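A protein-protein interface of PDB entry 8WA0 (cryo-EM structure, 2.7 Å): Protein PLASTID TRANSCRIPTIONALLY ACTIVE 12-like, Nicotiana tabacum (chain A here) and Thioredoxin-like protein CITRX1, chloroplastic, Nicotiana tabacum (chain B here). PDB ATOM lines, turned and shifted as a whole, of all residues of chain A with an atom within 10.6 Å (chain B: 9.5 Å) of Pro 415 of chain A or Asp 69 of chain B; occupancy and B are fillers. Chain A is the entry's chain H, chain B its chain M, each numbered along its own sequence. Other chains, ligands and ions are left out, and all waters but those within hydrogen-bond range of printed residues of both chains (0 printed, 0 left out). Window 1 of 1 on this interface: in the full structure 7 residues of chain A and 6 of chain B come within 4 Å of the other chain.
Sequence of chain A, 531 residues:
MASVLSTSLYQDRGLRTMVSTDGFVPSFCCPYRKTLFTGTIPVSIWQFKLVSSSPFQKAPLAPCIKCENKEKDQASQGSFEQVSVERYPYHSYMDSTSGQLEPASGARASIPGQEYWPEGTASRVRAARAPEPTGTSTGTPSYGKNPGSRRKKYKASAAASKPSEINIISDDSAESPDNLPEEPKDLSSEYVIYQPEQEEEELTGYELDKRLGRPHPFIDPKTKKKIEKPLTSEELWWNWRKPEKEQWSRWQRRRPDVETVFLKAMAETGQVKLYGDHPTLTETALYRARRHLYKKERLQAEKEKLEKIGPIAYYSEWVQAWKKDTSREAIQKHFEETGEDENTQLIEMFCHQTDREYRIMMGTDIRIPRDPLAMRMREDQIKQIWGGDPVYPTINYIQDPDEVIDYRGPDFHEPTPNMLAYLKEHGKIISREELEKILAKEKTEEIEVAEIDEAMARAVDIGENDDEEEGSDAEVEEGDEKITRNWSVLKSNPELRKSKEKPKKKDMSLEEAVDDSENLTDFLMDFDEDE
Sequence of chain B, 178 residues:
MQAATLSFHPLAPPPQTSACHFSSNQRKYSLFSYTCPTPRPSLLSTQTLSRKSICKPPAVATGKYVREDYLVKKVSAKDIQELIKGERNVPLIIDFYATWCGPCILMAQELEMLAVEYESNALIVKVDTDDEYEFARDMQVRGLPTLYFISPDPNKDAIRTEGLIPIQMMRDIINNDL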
ATOM      1  N   ASP A 406      21.053 -10.794  -8.002  1.00  0.00           N
ATOM      2  CA  ASP A 406      20.318  -9.923  -8.908  1.00  0.00           C
ATOM      3  C   ASP A 406      21.289  -9.270  -9.766  1.00  0.00           C
ATOM      4  O   ASP A 406      22.093  -8.500  -9.313  1.00  0.00           O
ATOM      5  CB  ASP A 406      19.556  -8.877  -8.173  1.00  0.00           C
ATOM      6  CG  ASP A 406      18.609  -8.114  -9.048  1.00  0.00           C
ATOM      7  OD1 ASP A 406      18.527  -8.406 -10.254  1.00  0.00           O
ATOM      8  OD2 ASP A 406      17.937  -7.212  -8.526  1.00  0.00           O
ATOM      9  N   TYR A 407      21.198  -9.538 -11.036  1.00  0.00           N
ATOM     10  CA  TYR A 407      22.158  -9.052 -11.928  1.00  0.00           C
ATOM     11  C   TYR A 407      21.900  -7.679 -12.373  1.00  0.00           C
ATOM     12  O   TYR A 407      22.758  -7.055 -12.937  1.00  0.00           O
ATOM     13  CB  TYR A 407      22.322 -10.023 -13.060  1.00  0.00           C
ATOM     14  CG  TYR A 407      22.992 -11.316 -12.731  1.00  0.00           C
ATOM     15  CD1 TYR A 407      24.162 -11.348 -12.012  1.00  0.00           C
ATOM     16  CD2 TYR A 407      22.474 -12.506 -13.184  1.00  0.00           C
ATOM     17  CE1 TYR A 407      24.786 -12.537 -11.729  1.00  0.00           C
ATOM     18  CE2 TYR A 407      23.094 -13.698 -12.909  1.00  0.00           C
ATOM     19  CZ  TYR A 407      24.246 -13.701 -12.180  1.00  0.00           C
ATOM     20  OH  TYR A 407      24.862 -14.883 -11.908  1.00  0.00           O
ATOM     21  N   ARG A 408      20.725  -7.182 -12.142  1.00  0.00           N
ATOM     22  CA  ARG A 408      20.455  -5.826 -12.446  1.00  0.00           C
ATOM     23  C   ARG A 408      20.589  -5.038 -11.192  1.00  0.00           C
ATOM     24  O   ARG A 408      19.611  -4.520 -10.709  1.00  0.00           O
ATOM     25  CB  ARG A 408      19.111  -5.758 -13.119  1.00  0.00           C
ATOM     26  CG  ARG A 408      19.064  -6.470 -14.442  1.00  0.00           C
ATOM     27  CD  ARG A 408      19.550  -5.542 -15.522  1.00  0.00           C
ATOM     28  NE  ARG A 408      18.565  -4.508 -15.733  1.00  0.00           N
ATOM     29  CZ  ARG A 408      18.827  -3.331 -16.260  1.00  0.00           C
ATOM     30  NH1 ARG A 408      17.859  -2.452 -16.398  1.00  0.00           N
ATOM     31  NH2 ARG A 408      20.056  -3.028 -16.630  1.00  0.00           N
ATOM     32  N   GLY A 409      21.771  -4.968 -10.619  1.00  0.00           N
ATOM     33  CA  GLY A 409      21.995  -4.325  -9.355  1.00  0.00           C
ATOM     34  C   GLY A 409      23.084  -3.342  -9.525  1.00  0.00           C
ATOM     35  O   GLY A 409      23.653  -3.280 -10.589  1.00  0.00           O
ATOM     36  N   ASP A 411      26.189  -3.015  -8.958  1.00  0.00           N
ATOM     37  CA  ASP A 411      27.583  -3.339  -9.216  1.00  0.00           C
ATOM     38  C   ASP A 411      27.860  -4.208 -10.412  1.00  0.00           C
ATOM     39  O   ASP A 411      28.935  -4.764 -10.524  1.00  0.00           O
ATOM     40  CB  ASP A 411      28.245  -3.908  -7.973  1.00  0.00           C
ATOM     41  CG  ASP A 411      27.504  -5.096  -7.391  1.00  0.00           C
ATOM     42  OD1 ASP A 411      26.259  -5.150  -7.464  1.00  0.00           O
ATOM     43  OD2 ASP A 411      28.179  -5.981  -6.824  1.00  0.00           O
ATOM     44  N   PHE A 412      26.901  -4.329 -11.312  1.00  0.00           N
ATOM     45  CA  PHE A 412      27.065  -5.179 -12.466  1.00  0.00           C
ATOM     46  C   PHE A 412      26.962  -4.395 -13.741  1.00  0.00           C
ATOM     47  O   PHE A 412      26.301  -3.379 -13.788  1.00  0.00           O
ATOM     48  CB  PHE A 412      26.020  -6.279 -12.476  1.00  0.00           C
ATOM     49  CG  PHE A 412      26.209  -7.320 -11.423  1.00  0.00           C
ATOM     50  CD1 PHE A 412      27.131  -8.327 -11.596  1.00  0.00           C
ATOM     51  CD2 PHE A 412      25.445  -7.305 -10.277  1.00  0.00           C
ATOM     52  CE1 PHE A 412      27.304  -9.293 -10.634  1.00  0.00           C
ATOM     53  CE2 PHE A 412      25.610  -8.268  -9.310  1.00  0.00           C
ATOM     54  CZ  PHE A 412      26.543  -9.263  -9.488  1.00  0.00           C
ATOM     55  N   HIS A 413      27.615  -4.866 -14.783  1.00  0.00           N
ATOM     56  CA  HIS A 413      27.596  -4.203 -16.071  1.00  0.00           C
ATOM     57  C   HIS A 413      26.284  -4.351 -16.771  1.00  0.00           C
ATOM     58  O   HIS A 413      25.490  -5.210 -16.430  1.00  0.00           O
ATOM     59  CB  HIS A 413      28.696  -4.750 -16.966  1.00  0.00           C
ATOM     60  CG  HIS A 413      28.622  -6.224 -17.202  1.00  0.00           C
ATOM     61  ND1 HIS A 413      27.831  -6.782 -18.181  1.00  0.00           N
ATOM     62  CD2 HIS A 413      29.266  -7.254 -16.608  1.00  0.00           C
ATOM     63  CE1 HIS A 413      27.975  -8.093 -18.167  1.00  0.00           C
ATOM     64  NE2 HIS A 413      28.842  -8.405 -17.221  1.00  0.00           N
ATOM     65  N   GLU A 414      26.040  -3.504 -17.751  1.00  0.00           N
ATOM     66  CA  GLU A 414      24.784  -3.537 -18.470  1.00  0.00           C
ATOM     67  C   GLU A 414      24.487  -4.861 -19.176  1.00  0.00           C
ATOM     68  O   GLU A 414      25.411  -5.542 -19.583  1.00  0.00           O
ATOM     69  CB  GLU A 414      24.717  -2.389 -19.451  1.00  0.00           C
ATOM     70  CG  GLU A 414      24.756  -1.028 -18.790  1.00  0.00           C
ATOM     71  CD  GLU A 414      23.526  -0.762 -17.956  1.00  0.00           C
ATOM     72  OE1 GLU A 414      22.408  -0.997 -18.458  1.00  0.00           O
ATOM     73  OE2 GLU A 414      23.673  -0.310 -16.804  1.00  0.00           O
ATOM     74  N   PRO A 415      23.198  -5.231 -19.360  1.00  0.00           N
ATOM     75  CA  PRO A 415      22.964  -6.530 -19.934  1.00  0.00           C
ATOM     76  C   PRO A 415      23.511  -6.708 -21.321  1.00  0.00           C
ATOM     77  O   PRO A 415      23.330  -5.822 -22.137  1.00  0.00           O
ATOM     78  CB  PRO A 415      21.465  -6.637 -19.858  1.00  0.00           C
ATOM     79  CG  PRO A 415      21.028  -5.711 -18.814  1.00  0.00           C
ATOM     80  CD  PRO A 415      21.959  -4.573 -18.942  1.00  0.00           C
ATOM     81  N   THR A 416      24.166  -7.816 -21.615  1.00  0.00           N
ATOM     82  CA  THR A 416      24.794  -8.064 -22.920  1.00  0.00           C
ATOM     83  C   THR A 416      23.864  -8.347 -24.038  1.00  0.00           C
ATOM     84  O   THR A 416      22.850  -8.988 -23.847  1.00  0.00           O
ATOM     85  CB  THR A 416      25.823  -9.193 -22.885  1.00  0.00           C
ATOM     86  OG1 THR A 416      25.154 -10.454 -22.822  1.00  0.00           O
ATOM     87  CG2 THR A 416      26.733  -9.043 -21.689  1.00  0.00           C
ATOM     88  N   PRO A 417      24.198  -7.893 -25.221  1.00  0.00           N
ATOM     89  CA  PRO A 417      23.303  -8.048 -26.343  1.00  0.00           C
ATOM     90  C   PRO A 417      23.705  -9.120 -27.362  1.00  0.00           C
ATOM     91  O   PRO A 417      24.893  -9.299 -27.585  1.00  0.00           O
ATOM     92  CB  PRO A 417      23.364  -6.685 -26.952  1.00  0.00           C
ATOM     93  CG  PRO A 417      24.585  -5.997 -26.443  1.00  0.00           C
ATOM     94  CD  PRO A 417      25.251  -6.912 -25.493  1.00  0.00           C
ATOM     95  N   ASN A 418      22.772  -9.822 -27.971  1.00  0.00           N
ATOM     96  CA  ASN A 418      23.089 -10.834 -28.929  1.00  0.00           C
ATOM     97  C   ASN A 418      23.724 -10.161 -30.088  1.00  0.00           C
ATOM     98  O   ASN A 418      23.232  -9.130 -30.522  1.00  0.00           O
ATOM     99  CB  ASN A 418      21.831 -11.544 -29.336  1.00  0.00           C
ATOM    100  CG  ASN A 418      22.094 -12.814 -30.097  1.00  0.00           C
ATOM    101  OD1 ASN A 418      23.226 -13.289 -30.174  1.00  0.00           O
ATOM    102  ND2 ASN A 418      21.043 -13.381 -30.659  1.00  0.00           N
ATOM    103  N   MET A 419      24.794 -10.694 -30.637  1.00  0.00           N
ATOM    104  CA  MET A 419      25.480  -9.986 -31.679  1.00  0.00           C
ATOM    105  C   MET A 419      24.585  -9.778 -32.850  1.00  0.00           C
ATOM    106  O   MET A 419      24.582  -8.714 -33.432  1.00  0.00           O
ATOM    107  CB  MET A 419      26.791 -10.643 -32.080  1.00  0.00           C
ATOM    108  CG  MET A 419      27.676  -9.835 -32.991  1.00  0.00           C
ATOM    109  SD  MET A 419      29.051  -9.097 -32.117  1.00  0.00           S
ATOM    110  CE  MET A 419      29.813 -10.547 -31.406  1.00  0.00           C
ATOM    111  N   TYR A 422      22.078  -6.873 -32.312  1.00  0.00           N
ATOM    112  CA  TYR A 422      22.742  -5.608 -32.270  1.00  0.00           C
ATOM    113  C   TYR A 422      23.131  -5.167 -33.623  1.00  0.00           C
ATOM    114  O   TYR A 422      22.925  -4.018 -33.985  1.00  0.00           O
ATOM    115  CB  TYR A 422      23.982  -5.763 -31.406  1.00  0.00           C
ATOM    116  CG  TYR A 422      24.750  -4.536 -31.038  1.00  0.00           C
ATOM    117  CD1 TYR A 422      24.297  -3.686 -30.055  1.00  0.00           C
ATOM    118  CD2 TYR A 422      25.969  -4.267 -31.621  1.00  0.00           C
ATOM    119  CE1 TYR A 422      25.017  -2.571 -29.696  1.00  0.00           C
ATOM    120  CE2 TYR A 422      26.695  -3.158 -31.273  1.00  0.00           C
ATOM    121  CZ  TYR A 422      26.215  -2.314 -30.307  1.00  0.00           C
ATOM    122  OH  TYR A 422      26.937  -1.200 -29.954  1.00  0.00           O
ATOM    123  N   GLU A 425      20.056  -4.071 -35.570  1.00  0.00           N
ATOM    124  CA  GLU A 425      19.529  -2.808 -35.120  1.00  0.00           C
ATOM    125  C   GLU A 425      20.274  -1.650 -35.679  1.00  0.00           C
ATOM    126  O   GLU A 425      19.683  -0.642 -36.005  1.00  0.00           O
ATOM    127  CB  GLU A 425      19.492  -2.734 -33.617  1.00  0.00           C
ATOM    128  CG  GLU A 425      18.668  -1.609 -33.039  1.00  0.00           C
ATOM    129  CD  GLU A 425      19.176  -1.176 -31.680  1.00  0.00           C
ATOM    130  OE1 GLU A 425      20.191  -1.744 -31.220  1.00  0.00           O
ATOM    131  OE2 GLU A 425      18.573  -0.266 -31.075  1.00  0.00           O
ATOM    132  N   GLY B  63      13.278   0.067 -31.217  1.00  0.00           N
ATOM    133  CA  GLY B  63      13.819  -0.977 -30.386  1.00  0.00           C
ATOM    134  C   GLY B  63      13.295  -2.278 -30.891  1.00  0.00           C
ATOM    135  O   GLY B  63      12.855  -3.123 -30.117  1.00  0.00           O
ATOM    136  N   TYR B  65      14.779  -4.937 -32.449  1.00  0.00           N
ATOM    137  CA  TYR B  65      15.459  -6.172 -32.212  1.00  0.00           C
ATOM    138  C   TYR B  65      16.021  -6.259 -30.839  1.00  0.00           C
ATOM    139  O   TYR B  65      16.096  -7.331 -30.269  1.00  0.00           O
ATOM    140  CB  TYR B  65      16.539  -6.345 -33.253  1.00  0.00           C
ATOM    141  CG  TYR B  65      16.055  -6.140 -34.666  1.00  0.00           C
ATOM    142  CD1 TYR B  65      15.177  -7.034 -35.253  1.00  0.00           C
ATOM    143  CD2 TYR B  65      16.481  -5.055 -35.413  1.00  0.00           C
ATOM    144  CE1 TYR B  65      14.730  -6.850 -36.542  1.00  0.00           C
ATOM    145  CE2 TYR B  65      16.041  -4.865 -36.705  1.00  0.00           C
ATOM    146  CZ  TYR B  65      15.166  -5.768 -37.262  1.00  0.00           C
ATOM    147  OH  TYR B  65      14.723  -5.583 -38.550  1.00  0.00           O
ATOM    148  N   VAL B  66      16.421  -5.136 -30.291  1.00  0.00           N
ATOM    149  CA  VAL B  66      16.907  -5.127 -28.956  1.00  0.00           C
ATOM    150  C   VAL B  66      15.950  -4.332 -28.123  1.00  0.00           C
ATOM    151  O   VAL B  66      15.556  -3.240 -28.493  1.00  0.00           O
ATOM    152  CB  VAL B  66      18.378  -4.693 -28.864  1.00  0.00           C
ATOM    153  CG1 VAL B  66      19.172  -5.173 -30.061  1.00  0.00           C
ATOM    154  CG2 VAL B  66      18.537  -3.192 -28.693  1.00  0.00           C
ATOM    155  N   ARG B  67      15.492  -4.897 -27.033  1.00  0.00           N
ATOM    156  CA  ARG B  67      14.565  -4.244 -26.172  1.00  0.00           C
ATOM    157  C   ARG B  67      15.277  -3.399 -25.174  1.00  0.00           C
ATOM    158  O   ARG B  67      16.287  -3.800 -24.629  1.00  0.00           O
ATOM    159  CB  ARG B  67      13.725  -5.297 -25.494  1.00  0.00           C
ATOM    160  CG  ARG B  67      12.779  -4.845 -24.402  1.00  0.00           C
ATOM    161  CD  ARG B  67      11.534  -4.204 -24.967  1.00  0.00           C
ATOM    162  NE  ARG B  67      10.543  -3.993 -23.926  1.00  0.00           N
ATOM    163  CZ  ARG B  67       9.427  -3.299 -24.092  1.00  0.00           C
ATOM    164  NH1 ARG B  67       9.167  -2.739 -25.263  1.00  0.00           N
ATOM    165  NH2 ARG B  67       8.577  -3.156 -23.086  1.00  0.00           N
ATOM    166  N   GLU B  68      14.765  -2.217 -24.922  1.00  0.00           N
ATOM    167  CA  GLU B  68      15.341  -1.326 -23.961  1.00  0.00           C
ATOM    168  C   GLU B  68      15.330  -1.803 -22.555  1.00  0.00           C
ATOM    169  O   GLU B  68      14.358  -2.352 -22.083  1.00  0.00           O
ATOM    170  CB  GLU B  68      14.569  -0.050 -24.013  1.00  0.00           C
ATOM    171  CG  GLU B  68      14.503   0.590 -25.390  1.00  0.00           C
ATOM    172  CD  GLU B  68      13.230   0.246 -26.144  1.00  0.00           C
ATOM    173  OE1 GLU B  68      12.360  -0.443 -25.569  1.00  0.00           O
ATOM    174  OE2 GLU B  68      13.101   0.667 -27.312  1.00  0.00           O
ATOM    175  N   ASP B  69      16.418  -1.603 -21.869  1.00  0.00           N
ATOM    176  CA  ASP B  69      16.548  -2.000 -20.508  1.00  0.00           C
ATOM    177  C   ASP B  69      15.754  -1.252 -19.519  1.00  0.00           C
ATOM    178  O   ASP B  69      15.276  -1.835 -18.573  1.00  0.00           O
ATOM    179  CB  ASP B  69      18.005  -1.970 -20.150  1.00  0.00           C
ATOM    180  CG  ASP B  69      18.877  -2.701 -21.143  1.00  0.00           C
ATOM    181  OD1 ASP B  69      18.361  -3.531 -21.918  1.00  0.00           O
ATOM    182  OD2 ASP B  69      20.097  -2.453 -21.143  1.00  0.00           O
ATOM    183  N   TYR B  70      15.596   0.048 -19.700  1.00  0.00           N
ATOM    184  CA  TYR B  70      14.971   0.858 -18.700  1.00  0.00           C
ATOM    185  C   TYR B  70      13.616   1.274 -19.132  1.00  0.00           C
ATOM    186  O   TYR B  70      13.451   1.775 -20.220  1.00  0.00           O
ATOM    187  CB  TYR B  70      15.904   2.011 -18.363  1.00  0.00           C
ATOM    188  CG  TYR B  70      17.277   1.627 -17.863  1.00  0.00           C
ATOM    189  CD1 TYR B  70      17.508   1.439 -16.530  1.00  0.00           C
ATOM    190  CD2 TYR B  70      18.344   1.497 -18.719  1.00  0.00           C
ATOM    191  CE1 TYR B  70      18.738   1.083 -16.051  1.00  0.00           C
ATOM    192  CE2 TYR B  70      19.588   1.152 -18.252  1.00  0.00           C
ATOM    193  CZ  TYR B  70      19.776   0.947 -16.917  1.00  0.00           C
ATOM    194  OH  TYR B  70      21.012   0.607 -16.434  1.00  0.00           O
ATOM    195  N   LEU B  71      12.625   1.049 -18.303  1.00  0.00           N
ATOM    196  CA  LEU B  71      11.252   1.309 -18.644  1.00  0.00           C
ATOM    197  C   LEU B  71      10.553   2.465 -17.998  1.00  0.00           C
ATOM    198  O   LEU B  71       9.362   2.603 -18.183  1.00  0.00           O
ATOM    199  CB  LEU B  71      10.440   0.065 -18.318  1.00  0.00           C
ATOM    200  CG  LEU B  71      10.400  -1.227 -19.137  1.00  0.00           C
ATOM    201  CD1 LEU B  71      11.752  -1.896 -19.323  1.00  0.00           C
ATOM    202  CD2 LEU B  71       9.446  -2.188 -18.465  1.00  0.00           C
ATOM    203  N   VAL B  72      11.247   3.294 -17.231  1.00  0.00           N
ATOM    204  CA  VAL B  72      10.675   4.463 -16.593  1.00  0.00           C
ATOM    205  C   VAL B  72      11.295   5.655 -17.268  1.00  0.00           C
ATOM    206  O   VAL B  72      12.490   5.674 -17.441  1.00  0.00           O
ATOM    207  CB  VAL B  72      10.861   4.395 -15.105  1.00  0.00           C
ATOM    208  CG1 VAL B  72      10.503   5.674 -14.394  1.00  0.00           C
ATOM    209  CG2 VAL B  72      10.260   3.137 -14.530  1.00  0.00           C
ATOM    210  N   LYS B  73      10.519   6.651 -17.676  1.00  0.00           N
ATOM    211  CA  LYS B  73      11.027   7.752 -18.472  1.00  0.00           C
ATOM    212  C   LYS B  73      11.055   9.129 -17.850  1.00  0.00           C
ATOM    213  O   LYS B  73      10.171   9.464 -17.102  1.00  0.00           O
ATOM    214  CB  LYS B  73      10.230   7.795 -19.754  1.00  0.00           C
ATOM    215  CG  LYS B  73      10.122   6.499 -20.529  1.00  0.00           C
ATOM    216  CD  LYS B  73      11.437   6.113 -21.176  1.00  0.00           C
ATOM    217  CE  LYS B  73      11.323   4.759 -21.852  1.00  0.00           C
ATOM    218  NZ  LYS B  73      12.631   4.294 -22.390  1.00  0.00           N
ATOM    219  N   ALA B 108      15.240   3.353  -7.461  1.00  0.00           N
ATOM    220  CA  ALA B 108      15.174   3.113  -8.857  1.00  0.00           C
ATOM    221  C   ALA B 108      14.966   1.691  -9.195  1.00  0.00           C
ATOM    222  O   ALA B 108      14.191   1.385 -10.081  1.00  0.00           O
ATOM    223  CB  ALA B 108      16.402   3.627  -9.483  1.00  0.00           C
ATOM    224  N   GLU B 112      11.367   0.281 -11.135  1.00  0.00           N
ATOM    225  CA  GLU B 112      11.416  -0.527 -12.323  1.00  0.00           C
ATOM    226  C   GLU B 112      10.670  -1.836 -12.175  1.00  0.00           C
ATOM    227  O   GLU B 112      10.072  -2.281 -13.140  1.00  0.00           O
ATOM    228  CB  GLU B 112      12.784  -0.657 -12.912  1.00  0.00           C
ATOM    229  CG  GLU B 112      13.201   0.486 -13.809  1.00  0.00           C
ATOM    230  CD  GLU B 112      14.548   0.254 -14.449  1.00  0.00           C
ATOM    231  OE1 GLU B 112      15.536   0.858 -13.982  1.00  0.00           O
ATOM    232  OE2 GLU B 112      14.623  -0.537 -15.413  1.00  0.00           O
ATOM    233  N   MET B 113      10.674  -2.490 -11.027  1.00  0.00           N
ATOM    234  CA  MET B 113       9.820  -3.673 -10.816  1.00  0.00           C
ATOM    235  C   MET B 113       8.333  -3.448 -10.814  1.00  0.00           C
ATOM    236  O   MET B 113       7.603  -4.264 -11.348  1.00  0.00           O
ATOM    237  CB  MET B 113      10.182  -4.475  -9.604  1.00  0.00           C
ATOM    238  CG  MET B 113      11.269  -5.497  -9.822  1.00  0.00           C
ATOM    239  SD  MET B 113      10.587  -7.005 -10.517  1.00  0.00           S
ATOM    240  CE  MET B 113       9.406  -7.444  -9.250  1.00  0.00           C
ATOM    241  N   ALA B 115       6.822  -1.373 -12.502  1.00  0.00           N
ATOM    242  CA  ALA B 115       6.493  -1.245 -13.884  1.00  0.00           C
ATOM    243  C   ALA B 115       6.280  -2.511 -14.625  1.00  0.00           C
ATOM    244  O   ALA B 115       5.374  -2.594 -15.423  1.00  0.00           O
ATOM    245  CB  ALA B 115       7.554  -0.460 -14.543  1.00  0.00           C
ATOM    246  N   VAL B 116       7.091  -3.515 -14.391  1.00  0.00           N
ATOM    247  CA  VAL B 116       6.933  -4.791 -15.029  1.00  0.00           C
ATOM    248  C   VAL B 116       5.639  -5.424 -14.623  1.00  0.00           C
ATOM    249  O   VAL B 116       4.963  -6.021 -15.441  1.00  0.00           O
ATOM    250  CB  VAL B 116       8.162  -5.681 -14.843  1.00  0.00           C
ATOM    251  CG1 VAL B 116       7.991  -7.008 -15.552  1.00  0.00           C
ATOM    252  CG2 VAL B 116       9.406  -4.975 -15.338  1.00  0.00           C
ATOM    253  N   LYS B 126       9.465   9.857 -14.099  1.00  0.00           N
ATOM    254  CA  LYS B 126      10.487  10.457 -13.247  1.00  0.00           C
ATOM    255  C   LYS B 126      10.957  11.891 -13.513  1.00  0.00           C
ATOM    256  O   LYS B 126      11.077  12.258 -14.640  1.00  0.00           O
ATOM    257  CB  LYS B 126      11.665   9.505 -13.112  1.00  0.00           C
ATOM    258  CG  LYS B 126      12.444   9.205 -14.361  1.00  0.00           C
ATOM    259  CD  LYS B 126      13.632   8.340 -14.017  1.00  0.00           C
ATOM    260  CE  LYS B 126      14.399   7.930 -15.251  1.00  0.00           C
ATOM    261  NZ  LYS B 126      15.488   6.993 -14.895  1.00  0.00           N
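The backbone carbonyl oxygen (O) of Asp 69 of chain B lies within hydrogen-bond range of the guanidinium group (NH1) of Arg 408 of chain A. The side-chain carboxylate of Glu 112 of chain B is in salt-bridge range of the guanidinium group of Arg 408 of chain A. The side-chain hydroxyl (OH) of Tyr 70 of chain B sits at hydrogen-bond distance from the side-chain carboxylate (OE2) of Glu 414 of chain A (2.8 Å).
The side-chain carboxylate (OD1) of Asp 406 of chain A sits at hydrogen-bond distance from the backbone NH (N) of Arg 408 of chain A (3.1 Å). The side-chain carboxylate (OE1) of Glu 414 of chain A is in salt-bridge range of the guanidinium group (NH2) of Arg 408 of chain A, at 3.6 Å. The side-chain amino group (NZ) of Lys 73 of chain B is in hydrogen-bond range of the backbone carbonyl oxygen (O) of Tyr 70 of chain B (3.4 Å).
Among the printed residues, merely in contact across the chains: Arg 408 of chain A with Tyr 70 of chain B (3.7 Å), Glu 414 of chain A with Asp 69 of chain B (3.8 Å), Pro 415 of chain A with Asp 69 of chain B (3.6 Å), Glu 425 of chain A with Tyr 65 of chain B (3.7 Å) and Glu 425 of chain A with Val 66 of chain B (3.3 Å).
Glu 414 of chain A touches just these residues of chain B: Asp 69 (3.8 Å) and Tyr 70 (2.8 Å). Pro 415 of chain A touches one residue of chain B. Thr 416 of chain A touches none of the printed residues of chain B. Printed residues of chain B within 4 Å of Glu 425 of chain A: Tyr 65 and Val 66. Of the printed residues of chain A, Val 66 of chain B touches Glu 425. Of chain A, only Arg 408 (3.4 Å), Glu 414 (3.8 Å) and Pro 415 (3.6 Å) come within 4 Å of Asp 69 of chain B. Tyr 70 of chain B touches just these residues of chain A: Arg 408 and Glu 414. Printed residues of chain A within 4 Å of Glu 112 of chain B: Arg 408. The nearest residue of chain A that does not touch Asp 69 of chain B is Thr 416 of chain A (6.7 Å).
Printed residues of chain A that touch a printed residue of chain B: Arg 408, Glu 414, Pro 415 and Glu 425. Among the printed residues, Asp or Glu carboxylates within 4 Å of a Lys or Arg side-chain nitrogen of the other chain: Arg 408 of chain A with Glu 112 of chain B.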
